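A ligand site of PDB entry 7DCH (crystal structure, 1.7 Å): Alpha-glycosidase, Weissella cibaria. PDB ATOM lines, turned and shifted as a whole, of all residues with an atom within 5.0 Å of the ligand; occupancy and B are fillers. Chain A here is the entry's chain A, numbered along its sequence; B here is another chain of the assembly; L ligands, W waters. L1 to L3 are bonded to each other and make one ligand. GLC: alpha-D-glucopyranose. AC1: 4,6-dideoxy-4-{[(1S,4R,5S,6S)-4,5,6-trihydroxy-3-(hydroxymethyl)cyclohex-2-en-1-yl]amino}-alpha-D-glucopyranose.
The side-chain carboxylate (OD2) of Asp 440 lies within hydrogen-bond range of an oxygen (O2) of GLC L2 (2.5 Å). OD2 of Asp 484 is in hydrogen-bond range of O3 of AC1 L3, at 2.7 Å. The side-chain amide oxygen of Gln 374 sits at hydrogen-bond distance from an oxygen (O3) of GLC L1 (2.7 Å). An oxygen (O6) of GLC L2 sits at hydrogen-bond distance from the side-chain carboxylate of Asp 345, at 2.8 Å. NH2 of Arg 488 sits at hydrogen-bond distance from O2 of AC1 L3 (2.9 Å). A ring nitrogen (NE2) of His 256 lies within hydrogen-bond range of an oxygen (O6) of GLC L2, 3.0 Å away. NH2 of Arg 343 lies within hydrogen-bond range of O2 of GLC L2, at 3.0 Å. NE2 of His 439 sits at hydrogen-bond distance from O3 of GLC L2 (3.1 Å). An oxygen (O5) of GLC L1 is in hydrogen-bond range of the guanidinium group (NH2) of Arg 49 of chain B, at 3.3 Å. OE2 of Glu 296 is in salt-bridge range of N4A of AC1 L3 (3.9 Å).
The side-chain carboxylate (OD2) of Asp 484 is in salt-bridge range of the guanidinium group (NH2) of Arg 488. The side-chain carboxylate (OD1) of Asp 345 sits close to the side-chain amide oxygen (OE1) of Gln 374 (3.3 Å). The side-chain carboxylate of Asp 345 is in salt-bridge range of the guanidinium group of Arg 343 (2.9 Å). O of His 439 lies within hydrogen-bond range of NH2 of Arg 488, 2.8 Å away. A ring nitrogen (NE2) of His 439 is in hydrogen-bond range of the side-chain hydroxyl (OH) of Tyr 216, 3.1 Å away. The backbone NH (N) of Glu 296 is in hydrogen-bond range of the side-chain amide oxygen (OD1) of Asn 294 (2.9 Å). N of Tyr 216 is in hydrogen-bond range of ND1 of His 214 (3.0 Å). The side-chain hydroxyl of Tyr 46 of chain B sits at hydrogen-bond distance from the side-chain carboxylate of Glu 349.
Residues that only touch the ligand: Val 346 (3.2 Å), Tyr 216 (3.3 Å), Met 312 (3.5 Å), Trp 376 (3.6 Å), Tyr 46 of chain B (3.6 Å), Phe 306 (3.6 Å) and His 214 (3.7 Å). Within 4 Å of the ligand: His 214, Tyr 216, His 256, Glu 296, Phe 306, Met 312, Arg 343, Asp 345, Val 346, Gln 374, Trp 376, His 439, Asp 440, Asp 484, Arg 488, Tyr 46 of chain B and Arg 49 of chain B. Along chain A the residues within 4 Å of the ligand span positions 214 to 488. The nearest printed residue that does not touch the ligand is Met 119 of chain B (4.2 Å).
Water W7 bridges O1 of GLC L1 (2.6 Å) and ND2 of Asn 120 of chain B (3.2 Å). Water W4 lies within hydrogen-bond range of O2 of GLC L1 (2.7 Å), OD1 of Asn 348 (2.8 Å) and O of Gln 374 (2.8 Å). Water W3 lies within hydrogen-bond range of O2 of GLC L1 (2.7 Å), OE2 of Glu 349 (2.8 Å), ND2 of Asn 348 (3.0 Å) and OH of Tyr 46 of chain B (3.3 Å). Water W5 bridges OD1 of Asn 120 of chain B (2.7 Å) and O1 of GLC L1 (3.0 Å). Water W1 lies within hydrogen-bond range of the side-chain carboxylate (OD2) of Asp 440 (2.7 Å), the indole nitrogen (NE1) of Trp 376 (3.1 Å), the side-chain amide nitrogen (NE2) of Gln 374 (3.1 Å) and an oxygen (O4) of GLC L1 (3.3 Å). Water W2 lies within hydrogen-bond range of OD2 of Asp 484 (2.8 Å) and OD1 of Asp 440 (2.8 Å).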
ATOM      1  N   ARG A 176      -9.889 -12.875  21.757  1.00  0.00           N
ATOM      2  CA  ARG A 176      -9.982 -12.912  20.302  1.00  0.00           C
ATOM      3  C   ARG A 176     -11.397 -12.639  19.819  1.00  0.00           C
ATOM      4  O   ARG A 176     -11.589 -12.090  18.720  1.00  0.00           O
ATOM      5  CB  ARG A 176      -9.506 -14.266  19.767  1.00  0.00           C
ATOM      6  CG  ARG A 176      -8.037 -14.606  20.067  1.00  0.00           C
ATOM      7  CD  ARG A 176      -7.893 -15.811  21.023  1.00  0.00           C
ATOM      8  NE  ARG A 176      -8.104 -15.470  22.438  1.00  0.00           N
ATOM      9  CZ  ARG A 176      -9.087 -15.941  23.194  1.00  0.00           C
ATOM     10  NH1 ARG A 176      -9.956 -16.818  22.696  1.00  0.00           N
ATOM     11  NH2 ARG A 176      -9.187 -15.573  24.459  1.00  0.00           N
ATOM     12  N   HIS A 214     -12.890  -8.141  13.770  1.00  0.00           N
ATOM     13  CA  HIS A 214     -11.911  -7.496  12.906  1.00  0.00           C
ATOM     14  C   HIS A 214     -12.381  -7.360  11.449  1.00  0.00           C
ATOM     15  O   HIS A 214     -11.914  -6.455  10.750  1.00  0.00           O
ATOM     16  CB  HIS A 214     -10.613  -8.289  12.937  1.00  0.00           C
ATOM     17  CG  HIS A 214     -10.795  -9.730  12.624  1.00  0.00           C
ATOM     18  ND1 HIS A 214     -10.923 -10.199  11.333  1.00  0.00           N
ATOM     19  CD2 HIS A 214     -10.828 -10.819  13.432  1.00  0.00           C
ATOM     20  CE1 HIS A 214     -11.062 -11.516  11.367  1.00  0.00           C
ATOM     21  NE2 HIS A 214     -10.990 -11.913  12.624  1.00  0.00           N
ATOM     22  N   TYR A 216     -12.045  -9.131   8.730  1.00  0.00           N
ATOM     23  CA  TYR A 216     -11.290  -9.592   7.573  1.00  0.00           C
ATOM     24  C   TYR A 216     -11.834 -10.874   6.970  1.00  0.00           C
ATOM     25  O   TYR A 216     -11.296 -11.356   5.965  1.00  0.00           O
ATOM     26  CB  TYR A 216      -9.809  -9.778   7.941  1.00  0.00           C
ATOM     27  CG  TYR A 216      -9.053  -8.472   8.056  1.00  0.00           C
ATOM     28  CD1 TYR A 216      -8.413  -7.932   6.940  1.00  0.00           C
ATOM     29  CD2 TYR A 216      -8.942  -7.806   9.282  1.00  0.00           C
ATOM     30  CE1 TYR A 216      -7.685  -6.758   7.037  1.00  0.00           C
ATOM     31  CE2 TYR A 216      -8.218  -6.634   9.388  1.00  0.00           C
ATOM     32  CZ  TYR A 216      -7.599  -6.112   8.261  1.00  0.00           C
ATOM     33  OH  TYR A 216      -6.895  -4.945   8.358  1.00  0.00           O
ATOM     34  N   VAL A 253     -10.119  -6.153   1.350  1.00  0.00           N
ATOM     35  CA  VAL A 253      -9.677  -7.493   1.711  1.00  0.00           C
ATOM     36  C   VAL A 253     -10.028  -8.388   0.545  1.00  0.00           C
ATOM     37  O   VAL A 253     -11.061  -9.073   0.562  1.00  0.00           O
ATOM     38  CB  VAL A 253     -10.350  -7.961   3.019  1.00  0.00           C
ATOM     39  CG1 VAL A 253      -9.763  -9.272   3.526  1.00  0.00           C
ATOM     40  CG2 VAL A 253     -10.242  -6.864   4.098  1.00  0.00           C
ATOM     41  N   HIS A 256      -8.945 -13.013   0.037  1.00  0.00           N
ATOM     42  CA  HIS A 256      -9.795 -14.082   0.503  1.00  0.00           C
ATOM     43  C   HIS A 256     -11.119 -13.479   0.921  1.00  0.00           C
ATOM     44  O   HIS A 256     -11.238 -12.268   1.130  1.00  0.00           O
ATOM     45  CB  HIS A 256      -9.142 -14.811   1.678  1.00  0.00           C
ATOM     46  CG  HIS A 256      -8.526 -13.882   2.691  1.00  0.00           C
ATOM     47  ND1 HIS A 256      -7.201 -13.487   2.627  1.00  0.00           N
ATOM     48  CD2 HIS A 256      -9.058 -13.286   3.790  1.00  0.00           C
ATOM     49  CE1 HIS A 256      -6.950 -12.664   3.637  1.00  0.00           C
ATOM     50  NE2 HIS A 256      -8.053 -12.556   4.374  1.00  0.00           N
ATOM     51  N   ASN A 294      -8.105 -25.156  17.550  1.00  0.00           N
ATOM     52  CA  ASN A 294      -7.795 -23.777  17.212  1.00  0.00           C
ATOM     53  C   ASN A 294      -8.692 -23.382  16.038  1.00  0.00           C
ATOM     54  O   ASN A 294      -8.553 -23.936  14.945  1.00  0.00           O
ATOM     55  CB  ASN A 294      -6.315 -23.650  16.847  1.00  0.00           C
ATOM     56  CG  ASN A 294      -5.922 -22.239  16.459  1.00  0.00           C
ATOM     57  OD1 ASN A 294      -6.764 -21.344  16.347  1.00  0.00           O
ATOM     58  ND2 ASN A 294      -4.615 -22.029  16.255  1.00  0.00           N
ATOM     59  N   GLU A 296      -8.621 -21.015  14.126  1.00  0.00           N
ATOM     60  CA  GLU A 296      -7.886 -20.421  13.011  1.00  0.00           C
ATOM     61  C   GLU A 296      -6.967 -21.404  12.276  1.00  0.00           C
ATOM     62  O   GLU A 296      -6.196 -20.971  11.411  1.00  0.00           O
ATOM     63  CB  GLU A 296      -7.054 -19.234  13.505  1.00  0.00           C
ATOM     64  CG  GLU A 296      -7.788 -18.244  14.376  1.00  0.00           C
ATOM     65  CD  GLU A 296      -8.670 -17.307  13.585  1.00  0.00           C
ATOM     66  OE1 GLU A 296      -9.011 -17.639  12.437  1.00  0.00           O
ATOM     67  OE2 GLU A 296      -9.010 -16.222  14.113  1.00  0.00           O
ATOM     68  N   PHE A 306      -6.204 -18.130   3.228  1.00  0.00           N
ATOM     69  CA  PHE A 306      -5.242 -17.319   3.947  1.00  0.00           C
ATOM     70  C   PHE A 306      -4.576 -18.188   5.011  1.00  0.00           C
ATOM     71  O   PHE A 306      -5.263 -18.935   5.713  1.00  0.00           O
ATOM     72  CB  PHE A 306      -5.887 -16.117   4.634  1.00  0.00           C
ATOM     73  CG  PHE A 306      -4.912 -15.353   5.470  1.00  0.00           C
ATOM     74  CD1 PHE A 306      -3.897 -14.633   4.857  1.00  0.00           C
ATOM     75  CD2 PHE A 306      -4.974 -15.392   6.855  1.00  0.00           C
ATOM     76  CE1 PHE A 306      -2.963 -13.933   5.604  1.00  0.00           C
ATOM     77  CE2 PHE A 306      -4.020 -14.697   7.630  1.00  0.00           C
ATOM     78  CZ  PHE A 306      -3.004 -13.956   6.978  1.00  0.00           C
ATOM     79  N   THR A 309      -6.080 -20.952   7.765  1.00  0.00           N
ATOM     80  CA  THR A 309      -7.392 -20.863   8.409  1.00  0.00           C
ATOM     81  C   THR A 309      -8.487 -21.279   7.434  1.00  0.00           C
ATOM     82  O   THR A 309      -8.644 -20.667   6.380  1.00  0.00           O
ATOM     83  CB  THR A 309      -7.700 -19.474   8.948  1.00  0.00           C
ATOM     84  OG1 THR A 309      -9.103 -19.453   9.266  1.00  0.00           O
ATOM     85  CG2 THR A 309      -7.404 -18.381   7.960  1.00  0.00           C
ATOM     86  N   MET A 312     -11.219 -18.605   5.733  1.00  0.00           N
ATOM     87  CA  MET A 312     -10.812 -17.572   4.779  1.00  0.00           C
ATOM     88  C   MET A 312     -10.343 -18.215   3.488  1.00  0.00           C
ATOM     89  O   MET A 312      -9.168 -18.118   3.120  1.00  0.00           O
ATOM     90  CB  MET A 312      -9.714 -16.683   5.378  1.00  0.00           C
ATOM     91  CG  MET A 312     -10.206 -15.843   6.558  1.00  0.00           C
ATOM     92  SD  MET A 312      -8.894 -14.826   7.246  1.00  0.00           S
ATOM     93  CE  MET A 312      -9.894 -13.737   8.288  1.00  0.00           C
ATOM     94  N   ARG A 343      -6.351   0.750   1.085  1.00  0.00           N
ATOM     95  CA  ARG A 343      -5.292  -0.076   1.668  1.00  0.00           C
ATOM     96  C   ARG A 343      -5.603  -1.527   1.315  1.00  0.00           C
ATOM     97  O   ARG A 343      -6.725  -1.998   1.543  1.00  0.00           O
ATOM     98  CB  ARG A 343      -5.198   0.154   3.172  1.00  0.00           C
ATOM     99  CG  ARG A 343      -4.108  -0.694   3.937  1.00  0.00           C
ATOM    100  CD  ARG A 343      -4.630  -2.037   4.425  1.00  0.00           C
ATOM    101  NE  ARG A 343      -3.799  -2.626   5.482  1.00  0.00           N
ATOM    102  CZ  ARG A 343      -3.915  -3.878   5.923  1.00  0.00           C
ATOM    103  NH1 ARG A 343      -4.841  -4.676   5.392  1.00  0.00           N
ATOM    104  NH2 ARG A 343      -3.120  -4.330   6.888  1.00  0.00           N
ATOM    105  N   ASP A 345      -5.233  -5.373   1.646  1.00  0.00           N
ATOM    106  CA  ASP A 345      -4.843  -6.464   2.540  1.00  0.00           C
ATOM    107  C   ASP A 345      -4.161  -7.607   1.790  1.00  0.00           C
ATOM    108  O   ASP A 345      -4.624  -8.026   0.723  1.00  0.00           O
ATOM    109  CB  ASP A 345      -6.101  -6.979   3.229  1.00  0.00           C
ATOM    110  CG  ASP A 345      -5.804  -7.963   4.340  1.00  0.00           C
ATOM    111  OD1 ASP A 345      -5.040  -7.583   5.258  1.00  0.00           O
ATOM    112  OD2 ASP A 345      -6.381  -9.076   4.320  1.00  0.00           O
ATOM    113  N   VAL A 346      -3.086  -8.156   2.385  1.00  0.00           N
ATOM    114  CA  VAL A 346      -2.312  -9.271   1.803  1.00  0.00           C
ATOM    115  C   VAL A 346      -2.115  -9.075   0.297  1.00  0.00           C
ATOM    116  O   VAL A 346      -2.306  -9.996  -0.509  1.00  0.00           O
ATOM    117  CB  VAL A 346      -2.991 -10.625   2.079  1.00  0.00           C
ATOM    118  CG1 VAL A 346      -1.915 -11.721   2.037  1.00  0.00           C
ATOM    119  CG2 VAL A 346      -3.718 -10.637   3.407  1.00  0.00           C
ATOM    120  N   ASN A 348       0.283  -8.841  -1.743  1.00  0.00           N
ATOM    121  CA  ASN A 348       1.304  -9.546  -2.497  1.00  0.00           C
ATOM    122  C   ASN A 348       0.815 -10.895  -3.001  1.00  0.00           C
ATOM    123  O   ASN A 348       1.400 -11.432  -3.942  1.00  0.00           O
ATOM    124  CB  ASN A 348       2.536  -9.729  -1.618  1.00  0.00           C
ATOM    125  CG  ASN A 348       2.214 -10.397  -0.268  1.00  0.00           C
ATOM    126  OD1 ASN A 348       1.091 -10.401   0.229  1.00  0.00           O
ATOM    127  ND2 ASN A 348       3.257 -10.900   0.364  1.00  0.00           N
ATOM    128  N   GLU A 349      -0.264 -11.427  -2.430  1.00  0.00           N
ATOM    129  CA  GLU A 349      -0.724 -12.756  -2.802  1.00  0.00           C
ATOM    130  C   GLU A 349      -1.791 -12.710  -3.896  1.00  0.00           C
ATOM    131  O   GLU A 349      -2.333 -13.764  -4.260  1.00  0.00           O
ATOM    132  CB  GLU A 349      -1.185 -13.513  -1.529  1.00  0.00           C
ATOM    133  CG  GLU A 349       0.013 -13.768  -0.597  1.00  0.00           C
ATOM    134  CD  GLU A 349      -0.331 -14.515   0.712  1.00  0.00           C
ATOM    135  OE1 GLU A 349      -1.429 -15.136   0.798  1.00  0.00           O
ATOM    136  OE2 GLU A 349       0.509 -14.476   1.644  1.00  0.00           O
ATOM    137  N   GLN A 374      -0.418  -3.709   1.423  1.00  0.00           N
ATOM    138  CA  GLN A 374       0.123  -4.230   2.670  1.00  0.00           C
ATOM    139  C   GLN A 374       1.051  -5.396   2.334  1.00  0.00           C
ATOM    140  O   GLN A 374       0.591  -6.516   2.100  1.00  0.00           O
ATOM    141  CB  GLN A 374      -0.960  -4.681   3.639  1.00  0.00           C
ATOM    142  CG  GLN A 374      -0.363  -5.080   5.011  1.00  0.00           C
ATOM    143  CD  GLN A 374      -1.057  -6.266   5.639  1.00  0.00           C
ATOM    144  OE1 GLN A 374      -1.848  -6.936   4.983  1.00  0.00           O
ATOM    145  NE2 GLN A 374      -0.764  -6.543   6.901  1.00  0.00           N
ATOM    146  N   TRP A 376       4.994  -6.971   3.605  1.00  0.00           N
ATOM    147  CA  TRP A 376       6.088  -6.908   4.595  1.00  0.00           C
ATOM    148  C   TRP A 376       7.483  -6.975   3.976  1.00  0.00           C
ATOM    149  O   TRP A 376       8.445  -6.546   4.620  1.00  0.00           O
ATOM    150  CB  TRP A 376       5.935  -8.064   5.585  1.00  0.00           C
ATOM    151  CG  TRP A 376       4.949  -7.821   6.678  1.00  0.00           C
ATOM    152  CD1 TRP A 376       3.594  -7.936   6.607  1.00  0.00           C
ATOM    153  CD2 TRP A 376       5.261  -7.477   8.033  1.00  0.00           C
ATOM    154  NE1 TRP A 376       3.037  -7.663   7.856  1.00  0.00           N
ATOM    155  CE2 TRP A 376       4.042  -7.365   8.737  1.00  0.00           C
ATOM    156  CE3 TRP A 376       6.454  -7.228   8.719  1.00  0.00           C
ATOM    157  CZ2 TRP A 376       3.979  -7.042  10.096  1.00  0.00           C
ATOM    158  CZ3 TRP A 376       6.398  -6.902  10.060  1.00  0.00           C
ATOM    159  CH2 TRP A 376       5.173  -6.801  10.738  1.00  0.00           C
ATOM    160  N   HIS A 439      -2.688  -2.840  14.356  1.00  0.00           N
ATOM    161  CA  HIS A 439      -3.603  -3.828  14.915  1.00  0.00           C
ATOM    162  C   HIS A 439      -3.033  -5.215  14.855  1.00  0.00           C
ATOM    163  O   HIS A 439      -3.707  -6.144  15.288  1.00  0.00           O
ATOM    164  CB  HIS A 439      -4.924  -3.802  14.153  1.00  0.00           C
ATOM    165  CG  HIS A 439      -4.768  -4.092  12.694  1.00  0.00           C
ATOM    166  ND1 HIS A 439      -3.958  -3.344  11.866  1.00  0.00           N
ATOM    167  CD2 HIS A 439      -5.296  -5.062  11.924  1.00  0.00           C
ATOM    168  CE1 HIS A 439      -4.014  -3.834  10.642  1.00  0.00           C
ATOM    169  NE2 HIS A 439      -4.829  -4.877  10.650  1.00  0.00           N
ATOM    170  N   ASP A 440      -1.832  -5.369  14.289  1.00  0.00           N
ATOM    171  CA  ASP A 440      -1.231  -6.687  14.185  1.00  0.00           C
ATOM    172  C   ASP A 440      -0.047  -6.875  15.110  1.00  0.00           C
ATOM    173  O   ASP A 440       0.243  -8.011  15.484  1.00  0.00           O
ATOM    174  CB  ASP A 440      -0.778  -6.962  12.744  1.00  0.00           C
ATOM    175  CG  ASP A 440      -1.938  -7.169  11.774  1.00  0.00           C
ATOM    176  OD1 ASP A 440      -3.007  -7.683  12.178  1.00  0.00           O
ATOM    177  OD2 ASP A 440      -1.775  -6.800  10.592  1.00  0.00           O
ATOM    178  N   ASP A 484      -1.800  -8.765  18.906  1.00  0.00           N
ATOM    179  CA  ASP A 484      -3.198  -9.121  18.644  1.00  0.00           C
ATOM    180  C   ASP A 484      -3.601 -10.365  19.429  1.00  0.00           C
ATOM    181  O   ASP A 484      -2.948 -11.412  19.275  1.00  0.00           O
ATOM    182  CB  ASP A 484      -3.338  -9.326  17.126  1.00  0.00           C
ATOM    183  CG  ASP A 484      -4.624 -10.012  16.700  1.00  0.00           C
ATOM    184  OD1 ASP A 484      -5.621 -10.010  17.452  1.00  0.00           O
ATOM    185  OD2 ASP A 484      -4.648 -10.575  15.576  1.00  0.00           O
ATOM    186  N   PRO A 485      -4.681 -10.327  20.252  1.00  0.00           N
ATOM    187  CA  PRO A 485      -5.683  -9.261  20.372  1.00  0.00           C
ATOM    188  C   PRO A 485      -5.400  -8.151  21.369  1.00  0.00           C
ATOM    189  O   PRO A 485      -6.222  -7.243  21.536  1.00  0.00           O
ATOM    190  CB  PRO A 485      -6.937 -10.022  20.844  1.00  0.00           C
ATOM    191  CG  PRO A 485      -6.361 -11.135  21.698  1.00  0.00           C
ATOM    192  CD  PRO A 485      -5.085 -11.559  20.962  1.00  0.00           C
ATOM    193  N   ARG A 488      -5.566  -4.279  20.677  1.00  0.00           N
ATOM    194  CA  ARG A 488      -6.856  -3.793  20.217  1.00  0.00           C
ATOM    195  C   ARG A 488      -7.747  -3.403  21.399  1.00  0.00           C
ATOM    196  O   ARG A 488      -8.958  -3.638  21.377  1.00  0.00           O
ATOM    197  CB  ARG A 488      -7.555  -4.833  19.341  1.00  0.00           C
ATOM    198  CG  ARG A 488      -6.793  -5.102  18.051  1.00  0.00           C
ATOM    199  CD  ARG A 488      -7.188  -6.422  17.425  1.00  0.00           C
ATOM    200  NE  ARG A 488      -6.329  -6.691  16.259  1.00  0.00           N
ATOM    201  CZ  ARG A 488      -6.596  -7.615  15.348  1.00  0.00           C
ATOM    202  NH1 ARG A 488      -7.719  -8.346  15.453  1.00  0.00           N
ATOM    203  NH2 ARG A 488      -5.764  -7.776  14.327  1.00  0.00           N
ATOM    204  N   TYR B  46       4.088 -19.517   5.760  1.00  0.00           N
ATOM    205  CA  TYR B  46       3.183 -19.648   6.885  1.00  0.00           C
ATOM    206  C   TYR B  46       3.412 -20.930   7.670  1.00  0.00           C
ATOM    207  O   TYR B  46       2.960 -21.060   8.818  1.00  0.00           O
ATOM    208  CB  TYR B  46       1.742 -19.598   6.372  1.00  0.00           C
ATOM    209  CG  TYR B  46       1.338 -18.254   5.789  1.00  0.00           C
ATOM    210  CD1 TYR B  46       0.807 -17.272   6.618  1.00  0.00           C
ATOM    211  CD2 TYR B  46       1.479 -17.972   4.435  1.00  0.00           C
ATOM    212  CE1 TYR B  46       0.434 -16.030   6.129  1.00  0.00           C
ATOM    213  CE2 TYR B  46       1.110 -16.732   3.915  1.00  0.00           C
ATOM    214  CZ  TYR B  46       0.578 -15.775   4.762  1.00  0.00           C
ATOM    215  OH  TYR B  46       0.181 -14.553   4.272  1.00  0.00           O
ATOM    216  N   ARG B  49       5.179 -20.592  11.536  1.00  0.00           N
ATOM    217  CA  ARG B  49       4.324 -20.232  12.673  1.00  0.00           C
ATOM    218  C   ARG B  49       3.171 -21.224  12.850  1.00  0.00           C
ATOM    219  O   ARG B  49       2.810 -21.570  13.981  1.00  0.00           O
ATOM    220  CB  ARG B  49       3.773 -18.793  12.489  1.00  0.00           C
ATOM    221  CG  ARG B  49       2.665 -18.475  11.353  1.00  0.00           C
ATOM    222  CD  ARG B  49       2.464 -16.912  11.115  1.00  0.00           C
ATOM    223  NE  ARG B  49       1.199 -16.560  10.452  1.00  0.00           N
ATOM    224  CZ  ARG B  49       0.809 -15.318  10.108  1.00  0.00           C
ATOM    225  NH1 ARG B  49       1.584 -14.266  10.335  1.00  0.00           N
ATOM    226  NH2 ARG B  49      -0.371 -15.145   9.518  1.00  0.00           N
ATOM    227  N   MET B 119       8.735 -15.346   9.017  1.00  0.00           N
ATOM    228  CA  MET B 119       8.549 -15.432   7.573  1.00  0.00           C
ATOM    229  C   MET B 119       9.021 -14.165   6.893  1.00  0.00           C
ATOM    230  O   MET B 119       9.420 -14.201   5.723  1.00  0.00           O
ATOM    231  CB  MET B 119       7.088 -15.727   7.210  1.00  0.00           C
ATOM    232  CG  MET B 119       6.065 -14.796   7.843  1.00  0.00           C
ATOM    233  SD  MET B 119       4.368 -15.387   7.510  1.00  0.00           S
ATOM    234  CE  MET B 119       4.082 -14.647   5.937  1.00  0.00           C
ATOM    235  N   ASN B 120       9.023 -13.037   7.612  1.00  0.00           N
ATOM    236  CA  ASN B 120       9.370 -11.776   6.959  1.00  0.00           C
ATOM    237  C   ASN B 120      10.879 -11.570   6.821  1.00  0.00           C
ATOM    238  O   ASN B 120      11.305 -10.577   6.215  1.00  0.00           O
ATOM    239  CB  ASN B 120       8.718 -10.630   7.732  1.00  0.00           C
ATOM    240  CG  ASN B 120       7.196 -10.735   7.685  1.00  0.00           C
ATOM    241  OD1 ASN B 120       6.654 -11.093   6.661  1.00  0.00           O
ATOM    242  ND2 ASN B 120       6.525 -10.436   8.797  1.00  0.00           N
HETATM  243  C1  GLC L   1       1.087 -11.958   6.999  1.00  0.00           C
HETATM  244  C2  GLC L   1       0.316 -11.311   5.832  1.00  0.00           C
HETATM  245  C3  GLC L   1      -0.475 -10.107   6.258  1.00  0.00           C
HETATM  246  C4  GLC L   1      -1.423 -10.475   7.355  1.00  0.00           C
HETATM  247  C5  GLC L   1      -0.634 -11.066   8.526  1.00  0.00           C
HETATM  248  C6  GLC L   1      -1.529 -11.521   9.620  1.00  0.00           C
HETATM  249  O1  GLC L   1       2.031 -11.064   7.463  1.00  0.00           O
HETATM  250  O2  GLC L   1       1.234 -10.935   4.778  1.00  0.00           O
HETATM  251  O3  GLC L   1      -1.167  -9.593   5.092  1.00  0.00           O
HETATM  252  O4  GLC L   1      -2.110  -9.341   7.929  1.00  0.00           O
HETATM  253  O5  GLC L   1       0.187 -12.250   8.147  1.00  0.00           O
HETATM  254  O6  GLC L   1      -0.662 -11.901  10.656  1.00  0.00           O
HETATM  255  C1  GLC L   2      -3.245  -8.904   7.285  1.00  0.00           C
HETATM  256  C2  GLC L   2      -4.060  -7.997   8.211  1.00  0.00           C
HETATM  257  C3  GLC L   2      -4.466  -8.830   9.398  1.00  0.00           C
HETATM  258  C4  GLC L   2      -5.441  -9.897   8.994  1.00  0.00           C
HETATM  259  C5  GLC L   2      -4.827 -10.800   7.917  1.00  0.00           C
HETATM  260  C6  GLC L   2      -5.864 -11.632   7.209  1.00  0.00           C
HETATM  261  O2  GLC L   2      -3.254  -6.858   8.559  1.00  0.00           O
HETATM  262  O3  GLC L   2      -5.045  -7.971  10.429  1.00  0.00           O
HETATM  263  O4  GLC L   2      -5.707 -10.686  10.143  1.00  0.00           O
HETATM  264  O5  GLC L   2      -4.096 -10.025   6.879  1.00  0.00           O
HETATM  265  O6  GLC L   2      -6.782 -10.814   6.507  1.00  0.00           O
HETATM  266  C1  AC1 L   3      -7.064 -10.838  10.456  1.00  0.00           C
HETATM  267  O2  AC1 L   3      -6.912  -9.096  12.073  1.00  0.00           O
HETATM  268  C2  AC1 L   3      -7.274 -10.475  11.916  1.00  0.00           C
HETATM  269  C4A AC1 L   3      -3.339 -15.036  15.890  1.00  0.00           C
HETATM  270  C3  AC1 L   3      -6.465 -11.347  12.817  1.00  0.00           C
HETATM  271  O3  AC1 L   3      -6.907 -11.061  14.189  1.00  0.00           O
HETATM  272  C4  AC1 L   3      -6.767 -12.779  12.524  1.00  0.00           C
HETATM  273  N4A AC1 L   3      -6.086 -13.738  13.462  1.00  0.00           N
HETATM  274  C5  AC1 L   3      -6.566 -13.144  11.028  1.00  0.00           C
HETATM  275  O5  AC1 L   3      -7.408 -12.233  10.206  1.00  0.00           O
HETATM  276  C6  AC1 L   3      -7.000 -14.542  10.732  1.00  0.00           C
HETATM  277  C1B AC1 L   3      -4.651 -13.935  13.402  1.00  0.00           C
HETATM  278  C2B AC1 L   3      -4.391 -15.593  13.638  1.00  0.00           C
HETATM  279  O2B AC1 L   3      -5.517 -16.285  13.024  1.00  0.00           O
HETATM  280  C3B AC1 L   3      -4.313 -16.011  14.895  1.00  0.00           C
HETATM  281  O3B AC1 L   3      -3.794 -17.380  14.958  1.00  0.00           O
HETATM  282  O4  AC1 L   3      -3.289 -15.550  17.177  1.00  0.00           O
HETATM  283  C5B AC1 L   3      -3.932 -13.754  15.905  1.00  0.00           C
HETATM  284  C7B AC1 L   3      -4.042 -13.138  14.437  1.00  0.00           C
HETATM  285  C6B AC1 L   3      -5.110 -13.586  16.881  1.00  0.00           C
HETATM  286  O6B AC1 L   3      -6.256 -14.169  16.307  1.00  0.00           O
HETATM  287  O   HOH W   1       0.406  -7.935   9.456  1.00  0.00           O
HETATM  288  O   HOH W   2      -2.818 -10.212  13.444  1.00  0.00           O
HETATM  289  O   HOH W   3       2.155 -12.416   2.723  1.00  0.00           O
HETATM  290  O   HOH W   4       1.115  -9.207   2.748  1.00  0.00           O
HETATM  291  O   HOH W   5       4.241 -11.240   5.391  1.00  0.00           O
HETATM  292  O   HOH W   6       3.884  -9.479   3.253  1.00  0.00           O
HETATM  293  O   HOH W   7       3.583 -11.381   9.547  1.00  0.00           O
